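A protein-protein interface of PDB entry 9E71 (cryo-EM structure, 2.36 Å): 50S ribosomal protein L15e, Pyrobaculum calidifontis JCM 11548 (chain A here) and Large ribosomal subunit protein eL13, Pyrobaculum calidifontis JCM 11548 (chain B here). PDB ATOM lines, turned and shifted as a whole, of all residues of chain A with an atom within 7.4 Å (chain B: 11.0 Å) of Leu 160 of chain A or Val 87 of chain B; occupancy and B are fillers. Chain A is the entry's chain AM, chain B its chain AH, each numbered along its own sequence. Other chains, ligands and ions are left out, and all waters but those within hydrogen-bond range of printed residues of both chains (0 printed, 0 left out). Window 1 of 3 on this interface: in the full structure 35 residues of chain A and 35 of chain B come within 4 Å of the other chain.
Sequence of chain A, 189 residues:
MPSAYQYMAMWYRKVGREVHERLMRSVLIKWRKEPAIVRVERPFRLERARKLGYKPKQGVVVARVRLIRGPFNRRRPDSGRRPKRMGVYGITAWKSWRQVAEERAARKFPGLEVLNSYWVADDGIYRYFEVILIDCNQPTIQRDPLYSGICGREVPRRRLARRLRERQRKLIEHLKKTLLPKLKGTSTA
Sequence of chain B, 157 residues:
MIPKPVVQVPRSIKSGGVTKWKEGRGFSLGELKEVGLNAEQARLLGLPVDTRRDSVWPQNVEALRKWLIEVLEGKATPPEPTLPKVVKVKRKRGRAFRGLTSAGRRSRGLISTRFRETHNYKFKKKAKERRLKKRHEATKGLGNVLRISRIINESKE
The backbone carbonyl oxygen (O) of Val 87 of chain B lies within hydrogen-bond range of the backbone NH (N) of Val 155 of chain A, at 3.2 Å.
The backbone carbonyl oxygen (O) of Arg 153 of chain A is in hydrogen-bond range of the backbone NH (N) of Val 89 of chain B (2.8 Å).
O of Arg 153 of chain A lies close to O of Val 87 of chain B (3.5 Å).
The side-chain amino group (NZ) of Lys 85 of chain B is in hydrogen-bond range of the backbone carbonyl oxygen (O) of Leu 83 of chain B.
Among the printed residues, merely in contact across the chains: Arg 153 of chain A with Lys 88 of chain B (3.8 Å), Glu 154 of chain A with Val 87 of chain B (3.4 Å), Arg 157 of chain A with Lys 85 of chain B (3.2 Å), Arg 157 of chain A with Val 86 of chain B (3.8 Å), Leu 160 of chain A with Pro 84 of chain B (3.8 Å), Leu 160 of chain A with Lys 85 of chain B (3.3 Å), Leu 160 of chain A with Val 86 of chain B (3.8 Å), Leu 160 of chain A with Val 87 of chain B (3.7 Å), Leu 164 of chain A with Pro 81 of chain B (3.9 Å) and Leu 164 of chain A with Leu 83 of chain B (3.7 Å).
Val 87 of chain B touches just these residues of chain A: Arg 153 (3.5 Å), Glu 154 (3.4 Å), Val 155 (3.2 Å) and Leu 160 (3.7 Å).
Arg 153 of chain A touches just these residues of chain B: Val 87 (3.5 Å), Lys 88 (3.8 Å) and Val 89 (2.8 Å).
No residue of chain B comes within 4 Å of Ala 161 of chain A.
Of the printed residues of chain A, Val 86 of chain B touches Arg 157 and Leu 160.
Of the printed residues of chain B, Arg 157 of chain A touches Lys 85 and Val 86.
Printed residues of chain A within 4 Å of Leu 83 of chain B: Leu 164.
Arg 43 of chain B touches none of the printed residues of chain A.
Arg 165 of chain A touches none of the printed residues of chain B.
The nearest residue of chain A that does not touch Val 87 of chain B is Pro 156 of chain A (6.0 Å).
Of the 14 printed residues of chain A, 6 touch a printed residue of chain B.
Among the printed residues, 13 pairs touch across the chains.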
ATOM      1  N   ARG A 153       4.905  12.377   6.155  1.00  0.00           N
ATOM      2  CA  ARG A 153       4.968  13.332   7.249  1.00  0.00           C
ATOM      3  C   ARG A 153       6.372  13.319   7.826  1.00  0.00           C
ATOM      4  O   ARG A 153       6.937  12.255   8.078  1.00  0.00           O
ATOM      5  CB  ARG A 153       3.945  13.004   8.336  1.00  0.00           C
ATOM      6  CG  ARG A 153       4.107  13.828   9.582  1.00  0.00           C
ATOM      7  CD  ARG A 153       2.968  13.595  10.543  1.00  0.00           C
ATOM      8  NE  ARG A 153       3.281  14.102  11.873  1.00  0.00           N
ATOM      9  CZ  ARG A 153       3.246  13.371  12.978  1.00  0.00           C
ATOM     10  NH1 ARG A 153       2.927  12.088  12.948  1.00  0.00           N
ATOM     11  NH2 ARG A 153       3.539  13.942  14.142  1.00  0.00           N
ATOM     12  N   GLU A 154       6.926  14.505   8.027  1.00  0.00           N
ATOM     13  CA  GLU A 154       8.258  14.657   8.585  1.00  0.00           C
ATOM     14  C   GLU A 154       8.196  15.623   9.751  1.00  0.00           C
ATOM     15  O   GLU A 154       7.413  16.575   9.739  1.00  0.00           O
ATOM     16  CB  GLU A 154       9.249  15.169   7.538  1.00  0.00           C
ATOM     17  CG  GLU A 154       9.225  16.677   7.322  1.00  0.00           C
ATOM     18  CD  GLU A 154       7.981  17.163   6.592  1.00  0.00           C
ATOM     19  OE1 GLU A 154       6.860  16.750   6.954  1.00  0.00           O
ATOM     20  OE2 GLU A 154       8.128  17.967   5.648  1.00  0.00           O
ATOM     21  N   VAL A 155       9.006  15.361  10.765  1.00  0.00           N
ATOM     22  CA  VAL A 155       9.191  16.273  11.882  1.00  0.00           C
ATOM     23  C   VAL A 155      10.690  16.468  12.056  1.00  0.00           C
ATOM     24  O   VAL A 155      11.434  15.484  12.116  1.00  0.00           O
ATOM     25  CB  VAL A 155       8.551  15.753  13.179  1.00  0.00           C
ATOM     26  CG1 VAL A 155       8.923  16.652  14.340  1.00  0.00           C
ATOM     27  CG2 VAL A 155       7.044  15.673  13.025  1.00  0.00           C
ATOM     28  N   PRO A 156      11.183  17.705  12.090  1.00  0.00           N
ATOM     29  CA  PRO A 156      12.617  17.928  12.318  1.00  0.00           C
ATOM     30  C   PRO A 156      13.035  17.412  13.685  1.00  0.00           C
ATOM     31  O   PRO A 156      12.333  17.601  14.681  1.00  0.00           O
ATOM     32  CB  PRO A 156      12.763  19.450  12.219  1.00  0.00           C
ATOM     33  CG  PRO A 156      11.535  19.921  11.519  1.00  0.00           C
ATOM     34  CD  PRO A 156      10.450  18.959  11.862  1.00  0.00           C
ATOM     35  N   ARG A 157      14.196  16.759  13.727  1.00  0.00           N
ATOM     36  CA  ARG A 157      14.631  16.120  14.962  1.00  0.00           C
ATOM     37  C   ARG A 157      14.979  17.141  16.033  1.00  0.00           C
ATOM     38  O   ARG A 157      14.934  16.818  17.226  1.00  0.00           O
ATOM     39  CB  ARG A 157      15.825  15.205  14.697  1.00  0.00           C
ATOM     40  CG  ARG A 157      15.963  14.085  15.704  1.00  0.00           C
ATOM     41  CD  ARG A 157      17.362  13.512  15.713  1.00  0.00           C
ATOM     42  NE  ARG A 157      18.320  14.402  16.352  1.00  0.00           N
ATOM     43  CZ  ARG A 157      18.813  14.222  17.568  1.00  0.00           C
ATOM     44  NH1 ARG A 157      18.453  13.192  18.315  1.00  0.00           N
ATOM     45  NH2 ARG A 157      19.692  15.095  18.048  1.00  0.00           N
ATOM     46  N   ARG A 158      15.321  18.368  15.632  1.00  0.00           N
ATOM     47  CA  ARG A 158      15.635  19.407  16.606  1.00  0.00           C
ATOM     48  C   ARG A 158      14.427  19.734  17.474  1.00  0.00           C
ATOM     49  O   ARG A 158      14.570  19.946  18.682  1.00  0.00           O
ATOM     50  CB  ARG A 158      16.173  20.654  15.891  1.00  0.00           C
ATOM     51  CG  ARG A 158      15.151  21.733  15.582  1.00  0.00           C
ATOM     52  CD  ARG A 158      15.491  22.495  14.338  1.00  0.00           C
ATOM     53  NE  ARG A 158      16.768  23.179  14.468  1.00  0.00           N
ATOM     54  CZ  ARG A 158      17.048  24.340  13.898  1.00  0.00           C
ATOM     55  NH1 ARG A 158      16.159  24.974  13.152  1.00  0.00           N
ATOM     56  NH2 ARG A 158      18.249  24.878  14.079  1.00  0.00           N
ATOM     57  N   ARG A 159      13.223  19.710  16.892  1.00  0.00           N
ATOM     58  CA  ARG A 159      12.014  20.024  17.642  1.00  0.00           C
ATOM     59  C   ARG A 159      11.757  18.990  18.730  1.00  0.00           C
ATOM     60  O   ARG A 159      11.611  19.331  19.914  1.00  0.00           O
ATOM     61  CB  ARG A 159      10.829  20.101  16.680  1.00  0.00           C
ATOM     62  CG  ARG A 159       9.745  21.072  17.087  1.00  0.00           C
ATOM     63  CD  ARG A 159       8.594  21.036  16.103  1.00  0.00           C
ATOM     64  NE  ARG A 159       8.918  21.733  14.867  1.00  0.00           N
ATOM     65  CZ  ARG A 159       8.145  21.747  13.790  1.00  0.00           C
ATOM     66  NH1 ARG A 159       6.986  21.114  13.763  1.00  0.00           N
ATOM     67  NH2 ARG A 159       8.546  22.414  12.713  1.00  0.00           N
ATOM     68  N   LEU A 160      11.740  17.712  18.346  1.00  0.00           N
ATOM     69  CA  LEU A 160      11.470  16.646  19.302  1.00  0.00           C
ATOM     70  C   LEU A 160      12.574  16.536  20.341  1.00  0.00           C
ATOM     71  O   LEU A 160      12.291  16.370  21.533  1.00  0.00           O
ATOM     72  CB  LEU A 160      11.288  15.319  18.567  1.00  0.00           C
ATOM     73  CG  LEU A 160      10.075  15.233  17.640  1.00  0.00           C
ATOM     74  CD1 LEU A 160       9.975  13.856  17.023  1.00  0.00           C
ATOM     75  CD2 LEU A 160       8.801  15.575  18.387  1.00  0.00           C
ATOM     76  N   ALA A 161      13.837  16.632  19.913  1.00  0.00           N
ATOM     77  CA  ALA A 161      14.948  16.515  20.849  1.00  0.00           C
ATOM     78  C   ALA A 161      14.957  17.659  21.850  1.00  0.00           C
ATOM     79  O   ALA A 161      15.164  17.437  23.047  1.00  0.00           O
ATOM     80  CB  ALA A 161      16.270  16.461  20.086  1.00  0.00           C
ATOM     81  N   ARG A 162      14.713  18.889  21.385  1.00  0.00           N
ATOM     82  CA  ARG A 162      14.699  20.031  22.287  1.00  0.00           C
ATOM     83  C   ARG A 162      13.554  19.931  23.284  1.00  0.00           C
ATOM     84  O   ARG A 162      13.743  20.165  24.484  1.00  0.00           O
ATOM     85  CB  ARG A 162      14.608  21.327  21.485  1.00  0.00           C
ATOM     86  CG  ARG A 162      14.387  22.565  22.334  1.00  0.00           C
ATOM     87  CD  ARG A 162      14.897  23.814  21.638  1.00  0.00           C
ATOM     88  NE  ARG A 162      14.031  24.211  20.536  1.00  0.00           N
ATOM     89  CZ  ARG A 162      13.705  25.464  20.252  1.00  0.00           C
ATOM     90  NH1 ARG A 162      14.158  26.477  20.972  1.00  0.00           N
ATOM     91  NH2 ARG A 162      12.903  25.707  19.219  1.00  0.00           N
ATOM     92  N   ARG A 163      12.356  19.574  22.808  1.00  0.00           N
ATOM     93  CA  ARG A 163      11.216  19.493  23.716  1.00  0.00           C
ATOM     94  C   ARG A 163      11.392  18.371  24.733  1.00  0.00           C
ATOM     95  O   ARG A 163      11.095  18.550  25.920  1.00  0.00           O
ATOM     96  CB  ARG A 163       9.923  19.316  22.924  1.00  0.00           C
ATOM     97  CG  ARG A 163       8.752  18.857  23.764  1.00  0.00           C
ATOM     98  CD  ARG A 163       8.025  20.023  24.423  1.00  0.00           C
ATOM     99  NE  ARG A 163       8.010  21.227  23.602  1.00  0.00           N
ATOM    100  CZ  ARG A 163       6.999  21.591  22.824  1.00  0.00           C
ATOM    101  NH1 ARG A 163       5.926  20.830  22.684  1.00  0.00           N
ATOM    102  NH2 ARG A 163       7.070  22.743  22.164  1.00  0.00           N
ATOM    103  N   LEU A 164      11.904  17.214  24.294  1.00  0.00           N
ATOM    104  CA  LEU A 164      12.142  16.111  25.219  1.00  0.00           C
ATOM    105  C   LEU A 164      13.216  16.458  26.242  1.00  0.00           C
ATOM    106  O   LEU A 164      13.084  16.119  27.423  1.00  0.00           O
ATOM    107  CB  LEU A 164      12.522  14.849  24.446  1.00  0.00           C
ATOM    108  CG  LEU A 164      11.364  13.972  23.961  1.00  0.00           C
ATOM    109  CD1 LEU A 164      11.865  12.772  23.174  1.00  0.00           C
ATOM    110  CD2 LEU A 164      10.509  13.515  25.128  1.00  0.00           C
ATOM    111  N   ARG A 165      14.289  17.132  25.811  1.00  0.00           N
ATOM    112  CA  ARG A 165      15.343  17.523  26.741  1.00  0.00           C
ATOM    113  C   ARG A 165      14.834  18.520  27.771  1.00  0.00           C
ATOM    114  O   ARG A 165      15.160  18.417  28.961  1.00  0.00           O
ATOM    115  CB  ARG A 165      16.523  18.111  25.971  1.00  0.00           C
ATOM    116  CG  ARG A 165      17.509  17.087  25.463  1.00  0.00           C
ATOM    117  CD  ARG A 165      18.829  17.736  25.094  1.00  0.00           C
ATOM    118  NE  ARG A 165      18.669  18.751  24.059  1.00  0.00           N
ATOM    119  CZ  ARG A 165      18.760  18.516  22.758  1.00  0.00           C
ATOM    120  NH1 ARG A 165      19.019  17.307  22.291  1.00  0.00           N
ATOM    121  NH2 ARG A 165      18.588  19.519  21.903  1.00  0.00           N
ATOM    122  N   GLU A 166      14.035  19.497  27.331  1.00  0.00           N
ATOM    123  CA  GLU A 166      13.464  20.466  28.260  1.00  0.00           C
ATOM    124  C   GLU A 166      12.529  19.792  29.256  1.00  0.00           C
ATOM    125  O   GLU A 166      12.557  20.102  30.456  1.00  0.00           O
ATOM    126  CB  GLU A 166      12.733  21.556  27.483  1.00  0.00           C
ATOM    127  CG  GLU A 166      12.102  22.621  28.351  1.00  0.00           C
ATOM    128  CD  GLU A 166      10.884  23.248  27.708  1.00  0.00           C
ATOM    129  OE1 GLU A 166      10.921  23.501  26.487  1.00  0.00           O
ATOM    130  OE2 GLU A 166       9.886  23.478  28.423  1.00  0.00           O
ATOM    131  N   ARG B  43      10.098   7.223  31.317  1.00  0.00           N
ATOM    132  CA  ARG B  43      10.629   7.341  29.966  1.00  0.00           C
ATOM    133  C   ARG B  43      11.312   8.683  29.760  1.00  0.00           C
ATOM    134  O   ARG B  43      12.293   8.778  29.015  1.00  0.00           O
ATOM    135  CB  ARG B  43       9.512   7.130  28.947  1.00  0.00           C
ATOM    136  CG  ARG B  43       9.106   5.677  28.808  1.00  0.00           C
ATOM    137  CD  ARG B  43       7.941   5.498  27.861  1.00  0.00           C
ATOM    138  NE  ARG B  43       7.583   4.091  27.723  1.00  0.00           N
ATOM    139  CZ  ARG B  43       6.342   3.638  27.636  1.00  0.00           C
ATOM    140  NH1 ARG B  43       5.304   4.456  27.653  1.00  0.00           N
ATOM    141  NH2 ARG B  43       6.136   2.329  27.528  1.00  0.00           N
ATOM    142  N   LEU B  44      10.810   9.734  30.415  1.00  0.00           N
ATOM    143  CA  LEU B  44      11.503  11.018  30.391  1.00  0.00           C
ATOM    144  C   LEU B  44      12.868  10.916  31.054  1.00  0.00           C
ATOM    145  O   LEU B  44      13.839  11.522  30.588  1.00  0.00           O
ATOM    146  CB  LEU B  44      10.652  12.085  31.076  1.00  0.00           C
ATOM    147  CG  LEU B  44       9.616  12.771  30.192  1.00  0.00           C
ATOM    148  CD1 LEU B  44       8.635  13.564  31.032  1.00  0.00           C
ATOM    149  CD2 LEU B  44      10.308  13.665  29.191  1.00  0.00           C
ATOM    150  N   GLU B  80      19.184  10.127  27.349  1.00  0.00           N
ATOM    151  CA  GLU B  80      18.089  10.796  26.669  1.00  0.00           C
ATOM    152  C   GLU B  80      16.802  10.000  26.877  1.00  0.00           C
ATOM    153  O   GLU B  80      16.850   8.794  27.132  1.00  0.00           O
ATOM    154  CB  GLU B  80      18.390  10.944  25.181  1.00  0.00           C
ATOM    155  CG  GLU B  80      17.925   9.777  24.336  1.00  0.00           C
ATOM    156  CD  GLU B  80      18.978   8.697  24.210  1.00  0.00           C
ATOM    157  OE1 GLU B  80      19.492   8.248  25.256  1.00  0.00           O
ATOM    158  OE2 GLU B  80      19.295   8.299  23.070  1.00  0.00           O
ATOM    159  N   PRO B  81      15.646  10.658  26.803  1.00  0.00           N
ATOM    160  CA  PRO B  81      14.383   9.983  27.137  1.00  0.00           C
ATOM    161  C   PRO B  81      14.053   8.862  26.163  1.00  0.00           C
ATOM    162  O   PRO B  81      14.379   8.925  24.978  1.00  0.00           O
ATOM    163  CB  PRO B  81      13.344  11.107  27.066  1.00  0.00           C
ATOM    164  CG  PRO B  81      14.104  12.376  26.964  1.00  0.00           C
ATOM    165  CD  PRO B  81      15.462  12.072  26.450  1.00  0.00           C
ATOM    166  N   THR B  82      13.397   7.825  26.685  1.00  0.00           N
ATOM    167  CA  THR B  82      13.024   6.655  25.893  1.00  0.00           C
ATOM    168  C   THR B  82      11.695   6.892  25.176  1.00  0.00           C
ATOM    169  O   THR B  82      10.695   6.212  25.397  1.00  0.00           O
ATOM    170  CB  THR B  82      12.958   5.416  26.777  1.00  0.00           C
ATOM    171  OG1 THR B  82      12.401   5.761  28.050  1.00  0.00           O
ATOM    172  CG2 THR B  82      14.339   4.827  26.977  1.00  0.00           C
ATOM    173  N   LEU B  83      11.705   7.881  24.295  1.00  0.00           N
ATOM    174  CA  LEU B  83      10.546   8.257  23.504  1.00  0.00           C
ATOM    175  C   LEU B  83      11.006   8.575  22.093  1.00  0.00           C
ATOM    176  O   LEU B  83      12.194   8.825  21.863  1.00  0.00           O
ATOM    177  CB  LEU B  83       9.814   9.455  24.121  1.00  0.00           C
ATOM    178  CG  LEU B  83       9.162   9.127  25.463  1.00  0.00           C
ATOM    179  CD1 LEU B  83       8.790  10.380  26.220  1.00  0.00           C
ATOM    180  CD2 LEU B  83       7.947   8.257  25.243  1.00  0.00           C
ATOM    181  N   PRO B  84      10.096   8.547  21.122  1.00  0.00           N
ATOM    182  CA  PRO B  84      10.498   8.752  19.723  1.00  0.00           C
ATOM    183  C   PRO B  84      11.012  10.163  19.479  1.00  0.00           C
ATOM    184  O   PRO B  84      10.315  11.149  19.720  1.00  0.00           O
ATOM    185  CB  PRO B  84       9.215   8.477  18.927  1.00  0.00           C
ATOM    186  CG  PRO B  84       8.189   8.052  19.884  1.00  0.00           C
ATOM    187  CD  PRO B  84       8.701   8.106  21.271  1.00  0.00           C
ATOM    188  N   LYS B  85      12.248  10.248  18.986  1.00  0.00           N
ATOM    189  CA  LYS B  85      12.883  11.520  18.685  1.00  0.00           C
ATOM    190  C   LYS B  85      12.802  11.907  17.219  1.00  0.00           C
ATOM    191  O   LYS B  85      13.139  13.044  16.879  1.00  0.00           O
ATOM    192  CB  LYS B  85      14.357  11.495  19.111  1.00  0.00           C
ATOM    193  CG  LYS B  85      14.589  10.949  20.505  1.00  0.00           C
ATOM    194  CD  LYS B  85      15.813  10.056  20.537  1.00  0.00           C
ATOM    195  CE  LYS B  85      15.793   9.129  21.739  1.00  0.00           C
ATOM    196  NZ  LYS B  85      14.775   8.051  21.602  1.00  0.00           N
ATOM    197  N   VAL B  86      12.381  10.999  16.343  1.00  0.00           N
ATOM    198  CA  VAL B  86      12.233  11.289  14.923  1.00  0.00           C
ATOM    199  C   VAL B  86      10.859  10.817  14.477  1.00  0.00           C
ATOM    200  O   VAL B  86      10.296   9.872  15.035  1.00  0.00           O
ATOM    201  CB  VAL B  86      13.334  10.617  14.074  1.00  0.00           C
ATOM    202  CG1 VAL B  86      13.430  11.282  12.716  1.00  0.00           C
ATOM    203  CG2 VAL B  86      14.673  10.666  14.789  1.00  0.00           C
ATOM    204  N   VAL B  87      10.315  11.485  13.466  1.00  0.00           N
ATOM    205  CA  VAL B  87       9.054  11.093  12.848  1.00  0.00           C
ATOM    206  C   VAL B  87       9.266  11.148  11.343  1.00  0.00           C
ATOM    207  O   VAL B  87       9.149  12.212  10.730  1.00  0.00           O
ATOM    208  CB  VAL B  87       7.885  11.986  13.271  1.00  0.00           C
ATOM    209  CG1 VAL B  87       6.603  11.514  12.609  1.00  0.00           C
ATOM    210  CG2 VAL B  87       7.742  11.991  14.782  1.00  0.00           C
ATOM    211  N   LYS B  88       9.566  10.006  10.741  1.00  0.00           N
ATOM    212  CA  LYS B  88       9.797   9.905   9.305  1.00  0.00           C
ATOM    213  C   LYS B  88       8.709   9.009   8.725  1.00  0.00           C
ATOM    214  O   LYS B  88       8.732   7.792   8.920  1.00  0.00           O
ATOM    215  CB  LYS B  88      11.189   9.355   9.021  1.00  0.00           C
ATOM    216  CG  LYS B  88      11.692   9.611   7.619  1.00  0.00           C
ATOM    217  CD  LYS B  88      13.039   8.948   7.400  1.00  0.00           C
ATOM    218  CE  LYS B  88      13.755   8.712   8.721  1.00  0.00           C
ATOM    219  NZ  LYS B  88      15.087   8.074   8.540  1.00  0.00           N
ATOM    220  N   VAL B  89       7.752   9.608   8.023  1.00  0.00           N
ATOM    221  CA  VAL B  89       6.680   8.876   7.361  1.00  0.00           C
ATOM    222  C   VAL B  89       6.800   9.119   5.865  1.00  0.00           C
ATOM    223  O   VAL B  89       6.717  10.265   5.410  1.00  0.00           O
ATOM    224  CB  VAL B  89       5.296   9.292   7.878  1.00  0.00           C
ATOM    225  CG1 VAL B  89       4.217   8.430   7.244  1.00  0.00           C
ATOM    226  CG2 VAL B  89       5.246   9.182   9.381  1.00  0.00           C
ATOM    227  N   LYS B  90       6.986   8.046   5.102  1.00  0.00           N
ATOM    228  CA  LYS B  90       7.162   8.159   3.663  1.00  0.00           C
ATOM    229  C   LYS B  90       5.821   8.142   2.946  1.00  0.00           C
ATOM    230  O   LYS B  90       4.875   7.482   3.382  1.00  0.00           O
ATOM    231  CB  LYS B  90       8.037   7.022   3.140  1.00  0.00           C
ATOM    232  CG  LYS B  90       9.519   7.231   3.358  1.00  0.00           C
ATOM    233  CD  LYS B  90      10.334   6.191   2.624  1.00  0.00           C
ATOM    234  CE  LYS B  90      11.798   6.281   2.991  1.00  0.00           C
ATOM    235  NZ  LYS B  90      12.553   5.112   2.480  1.00  0.00           N
ATOM    236  N   ARG B  91       5.746   8.878   1.842  1.00  0.00           N
ATOM    237  CA  ARG B  91       4.587   8.807   0.964  1.00  0.00           C
ATOM    238  C   ARG B  91       4.466   7.406   0.380  1.00  0.00           C
ATOM    239  O   ARG B  91       5.451   6.829  -0.085  1.00  0.00           O
ATOM    240  CB  ARG B  91       4.713   9.849  -0.147  1.00  0.00           C
ATOM    241  CG  ARG B  91       3.911   9.560  -1.405  1.00  0.00           C
ATOM    242  CD  ARG B  91       2.420   9.526  -1.142  1.00  0.00           C
ATOM    243  NE  ARG B  91       1.699   8.828  -2.199  1.00  0.00           N
ATOM    244  CZ  ARG B  91       1.426   9.346  -3.389  1.00  0.00           C
ATOM    245  NH1 ARG B  91       1.794  10.578  -3.707  1.00  0.00           N
ATOM    246  NH2 ARG B  91       0.761   8.614  -4.279  1.00  0.00           N
ATOM    247  N   LYS B  92       3.256   6.859   0.405  1.00  0.00           N
ATOM    248  CA  LYS B  92       3.003   5.492  -0.029  1.00  0.00           C
ATOM    249  C   LYS B  92       2.471   5.502  -1.456  1.00  0.00           C
ATOM    250  O   LYS B  92       1.429   6.102  -1.729  1.00  0.00           O
ATOM    251  CB  LYS B  92       2.012   4.803   0.907  1.00  0.00           C
ATOM    252  CG  LYS B  92       2.297   5.027   2.376  1.00  0.00           C
ATOM    253  CD  LYS B  92       3.474   4.196   2.834  1.00  0.00           C
ATOM    254  CE  LYS B  92       3.700   4.337   4.322  1.00  0.00           C
ATOM    255  NZ  LYS B  92       3.546   5.741   4.767  1.00  0.00           N
